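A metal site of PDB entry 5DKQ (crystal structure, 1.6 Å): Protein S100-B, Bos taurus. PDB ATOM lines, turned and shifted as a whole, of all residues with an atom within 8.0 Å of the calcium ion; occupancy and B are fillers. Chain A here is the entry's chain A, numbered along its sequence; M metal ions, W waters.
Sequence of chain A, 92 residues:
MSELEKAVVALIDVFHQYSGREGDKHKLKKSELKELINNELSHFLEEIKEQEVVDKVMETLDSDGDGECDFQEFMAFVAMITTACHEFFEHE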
ATOM      1  N   LYS A  27      -9.129  11.574  13.618  1.00  0.00           N
ATOM      2  CA  LYS A  27      -9.491  12.654  14.508  1.00  0.00           C
ATOM      3  C   LYS A  27      -8.783  13.944  14.115  1.00  0.00           C
ATOM      4  O   LYS A  27      -7.669  13.920  13.559  1.00  0.00           O
ATOM      5  CB  LYS A  27      -9.174  12.295  15.975  1.00  0.00           C
ATOM      6  CG  LYS A  27      -9.877  11.067  16.522  1.00  0.00           C
ATOM      7  CD  LYS A  27      -9.515  10.835  17.981  1.00  0.00           C
ATOM      8  CE  LYS A  27     -10.143   9.573  18.520  1.00  0.00           C
ATOM      9  NZ  LYS A  27      -9.788   8.373  17.722  1.00  0.00           N
ATOM     10  N   LEU A  28      -9.442  15.073  14.374  1.00  0.00           N
ATOM     11  CA  LEU A  28      -8.805  16.359  14.202  1.00  0.00           C
ATOM     12  C   LEU A  28      -8.148  16.764  15.526  1.00  0.00           C
ATOM     13  O   LEU A  28      -8.834  16.973  16.532  1.00  0.00           O
ATOM     14  CB  LEU A  28      -9.831  17.431  13.823  1.00  0.00           C
ATOM     15  CG  LEU A  28     -10.629  17.241  12.540  1.00  0.00           C
ATOM     16  CD1 LEU A  28     -11.930  18.045  12.630  1.00  0.00           C
ATOM     17  CD2 LEU A  28      -9.816  17.698  11.326  1.00  0.00           C
ATOM     18  N   MET A  58     -11.949  23.831  20.508  1.00  0.00           N
ATOM     19  CA  MET A  58     -11.784  22.414  20.811  1.00  0.00           C
ATOM     20  C   MET A  58     -12.426  22.025  22.140  1.00  0.00           C
ATOM     21  O   MET A  58     -12.992  20.935  22.249  1.00  0.00           O
ATOM     22  CB  MET A  58     -10.307  22.008  20.797  1.00  0.00           C
ATOM     23  CG  MET A  58     -10.104  20.513  21.032  1.00  0.00           C
ATOM     24  SD  MET A  58     -10.762  19.460  19.688  1.00  0.00           S
ATOM     25  CE  MET A  58      -9.457  19.604  18.476  1.00  0.00           C
ATOM     26  N   LEU A  61     -15.985  21.518  21.425  1.00  0.00           N
ATOM     27  CA  LEU A  61     -16.261  20.351  20.581  1.00  0.00           C
ATOM     28  C   LEU A  61     -15.922  18.988  21.174  1.00  0.00           C
ATOM     29  O   LEU A  61     -16.539  17.987  20.828  1.00  0.00           O
ATOM     30  CB  LEU A  61     -15.532  20.487  19.237  1.00  0.00           C
ATOM     31  CG  LEU A  61     -15.875  21.678  18.357  1.00  0.00           C
ATOM     32  CD1 LEU A  61     -15.195  21.507  17.011  1.00  0.00           C
ATOM     33  CD2 LEU A  61     -17.390  21.811  18.194  1.00  0.00           C
ATOM     34  N   ASP A  62     -14.917  18.953  22.052  1.00  0.00           N
ATOM     35  CA  ASP A  62     -14.383  17.678  22.547  1.00  0.00           C
ATOM     36  C   ASP A  62     -15.208  17.111  23.691  1.00  0.00           C
ATOM     37  O   ASP A  62     -14.930  17.378  24.850  1.00  0.00           O
ATOM     38  CB  ASP A  62     -12.921  17.873  22.976  1.00  0.00           C
ATOM     39  CG  ASP A  62     -12.293  16.631  23.542  1.00  0.00           C
ATOM     40  OD1 ASP A  62     -12.744  15.523  23.185  1.00  0.00           O
ATOM     41  OD2 ASP A  62     -11.334  16.739  24.339  1.00  0.00           O
ATOM     42  N   SER A  63     -16.214  16.295  23.381  1.00  0.00           N
ATOM     43  CA  SER A  63     -17.125  15.791  24.403  1.00  0.00           C
ATOM     44  C   SER A  63     -16.618  14.571  25.185  1.00  0.00           C
ATOM     45  O   SER A  63     -17.248  14.159  26.157  1.00  0.00           O
ATOM     46  CB  SER A  63     -18.492  15.480  23.806  1.00  0.00           C
ATOM     47  OG  SER A  63     -19.102  16.648  23.272  1.00  0.00           O
ATOM     48  N   ASP A  64     -15.513  13.964  24.767  1.00  0.00           N
ATOM     49  CA  ASP A  64     -14.999  12.802  25.496  1.00  0.00           C
ATOM     50  C   ASP A  64     -13.616  13.025  26.107  1.00  0.00           C
ATOM     51  O   ASP A  64     -12.962  12.075  26.542  1.00  0.00           O
ATOM     52  CB  ASP A  64     -15.014  11.531  24.638  1.00  0.00           C
ATOM     53  CG  ASP A  64     -14.068  11.618  23.438  1.00  0.00           C
ATOM     54  OD1 ASP A  64     -13.445  12.670  23.228  1.00  0.00           O
ATOM     55  OD2 ASP A  64     -13.965  10.608  22.697  1.00  0.00           O
ATOM     56  N   GLY A  65     -13.180  14.282  26.125  1.00  0.00           N
ATOM     57  CA  GLY A  65     -11.987  14.696  26.842  1.00  0.00           C
ATOM     58  C   GLY A  65     -10.635  14.250  26.316  1.00  0.00           C
ATOM     59  O   GLY A  65      -9.640  14.340  27.042  1.00  0.00           O
ATOM     60  N   ASP A  66     -10.570  13.784  25.079  1.00  0.00           N
ATOM     61  CA  ASP A  66      -9.306  13.282  24.531  1.00  0.00           C
ATOM     62  C   ASP A  66      -8.482  14.363  23.822  1.00  0.00           C
ATOM     63  O   ASP A  66      -7.389  14.106  23.299  1.00  0.00           O
ATOM     64  CB  ASP A  66      -9.538  12.076  23.629  1.00  0.00           C
ATOM     65  CG  ASP A  66     -10.170  12.443  22.307  1.00  0.00           C
ATOM     66  OD1 ASP A  66     -10.637  13.589  22.143  1.00  0.00           O
ATOM     67  OD2 ASP A  66     -10.190  11.567  21.422  1.00  0.00           O
ATOM     68  N   GLY A  67      -9.009  15.588  23.818  1.00  0.00           N
ATOM     69  CA  GLY A  67      -8.288  16.742  23.304  1.00  0.00           C
ATOM     70  C   GLY A  67      -8.369  16.887  21.793  1.00  0.00           C
ATOM     71  O   GLY A  67      -7.727  17.767  21.204  1.00  0.00           O
ATOM     72  N   GLU A  68      -9.161  16.022  21.170  1.00  0.00           N
ATOM     73  CA  GLU A  68      -9.276  15.996  19.719  1.00  0.00           C
ATOM     74  C   GLU A  68     -10.737  15.956  19.308  1.00  0.00           C
ATOM     75  O   GLU A  68     -11.607  15.640  20.114  1.00  0.00           O
ATOM     76  CB  GLU A  68      -8.543  14.772  19.160  1.00  0.00           C
ATOM     77  CG  GLU A  68      -7.037  14.739  19.497  1.00  0.00           C
ATOM     78  CD  GLU A  68      -6.196  14.049  18.441  1.00  0.00           C
ATOM     79  OE1 GLU A  68      -6.647  13.922  17.277  1.00  0.00           O
ATOM     80  OE2 GLU A  68      -5.055  13.644  18.780  1.00  0.00           O
ATOM     81  N   CYS A  69     -11.007  16.268  18.047  1.00  0.00           N
ATOM     82  CA  CYS A  69     -12.373  16.214  17.557  1.00  0.00           C
ATOM     83  C   CYS A  69     -12.545  14.989  16.641  1.00  0.00           C
ATOM     84  O   CYS A  69     -11.963  14.947  15.554  1.00  0.00           O
ATOM     85  CB  CYS A  69     -12.673  17.496  16.792  1.00  0.00           C
ATOM     86  SG  CYS A  69     -14.351  17.590  16.102  1.00  0.00           S
ATOM     87  N   ASP A  70     -13.347  14.006  17.073  1.00  0.00           N
ATOM     88  CA  ASP A  70     -13.592  12.809  16.244  1.00  0.00           C
ATOM     89  C   ASP A  70     -14.749  13.065  15.272  1.00  0.00           C
ATOM     90  O   ASP A  70     -15.249  14.184  15.177  1.00  0.00           O
ATOM     91  CB  ASP A  70     -13.771  11.518  17.080  1.00  0.00           C
ATOM     92  CG  ASP A  70     -15.040  11.500  17.921  1.00  0.00           C
ATOM     93  OD1 ASP A  70     -15.941  12.341  17.708  1.00  0.00           O
ATOM     94  OD2 ASP A  70     -15.157  10.595  18.779  1.00  0.00           O
ATOM     95  N   PHE A  71     -15.146  12.053  14.497  1.00  0.00           N
ATOM     96  CA  PHE A  71     -16.175  12.276  13.492  1.00  0.00           C
ATOM     97  C   PHE A  71     -17.506  12.705  14.093  1.00  0.00           C
ATOM     98  O   PHE A  71     -18.151  13.630  13.603  1.00  0.00           O
ATOM     99  CB  PHE A  71     -16.375  11.068  12.574  1.00  0.00           C
ATOM    100  CG  PHE A  71     -17.240  11.378  11.385  1.00  0.00           C
ATOM    101  CD1 PHE A  71     -16.707  12.048  10.294  1.00  0.00           C
ATOM    102  CD2 PHE A  71     -18.577  11.028  11.367  1.00  0.00           C
ATOM    103  CE1 PHE A  71     -17.483  12.350   9.188  1.00  0.00           C
ATOM    104  CE2 PHE A  71     -19.364  11.323  10.257  1.00  0.00           C
ATOM    105  CZ  PHE A  71     -18.821  11.987   9.174  1.00  0.00           C
ATOM    106  N   GLU A  73     -18.039  14.170  16.924  1.00  0.00           N
ATOM    107  CA  GLU A  73     -17.884  15.525  17.438  1.00  0.00           C
ATOM    108  C   GLU A  73     -17.860  16.548  16.299  1.00  0.00           C
ATOM    109  O   GLU A  73     -18.333  17.677  16.440  1.00  0.00           O
ATOM    110  CB  GLU A  73     -16.631  15.603  18.323  1.00  0.00           C
ATOM    111  CG  GLU A  73     -16.773  14.789  19.631  1.00  0.00           C
ATOM    112  CD  GLU A  73     -15.434  14.486  20.304  1.00  0.00           C
ATOM    113  OE1 GLU A  73     -14.397  14.576  19.631  1.00  0.00           O
ATOM    114  OE2 GLU A  73     -15.416  14.144  21.516  1.00  0.00           O
HETATM  115 CA    CA M   1     -12.853  14.048  21.461  1.00  0.00          CA
HETATM  116  O   HOH W   1     -12.440  12.025  20.195  1.00  0.00           O
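N of Glu 73 sits at hydrogen-bond distance from OD1 of Asp 70 (2.9 Å). The side-chain carboxylate of Asp 62 sits at hydrogen-bond distance from the backbone NH of Gly 67 (2.6 Å). The side-chain carboxylate (OD1) of Asp 62 sits close to the backbone NH (N) of Gly 65, 3.2 Å away. OE2 of Glu 73 lies close to N of Ser 63, at 3.0 Å.
Within 4 Å of the calcium ion: Asp 62, Asp 64, Asp 66, Glu 68 and Glu 73.
The calcium ion is bound by OD1 of Asp 62 (2.3 Å), OD1 of Asp 64 (2.3 Å), OD1 of Asp 66 (2.4 Å), water W1 (2.4 Å), O of Glu 68 (2.4 Å), OE1 of Glu 73 (2.5 Å) and OE2 of Glu 73 (2.6 Å).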
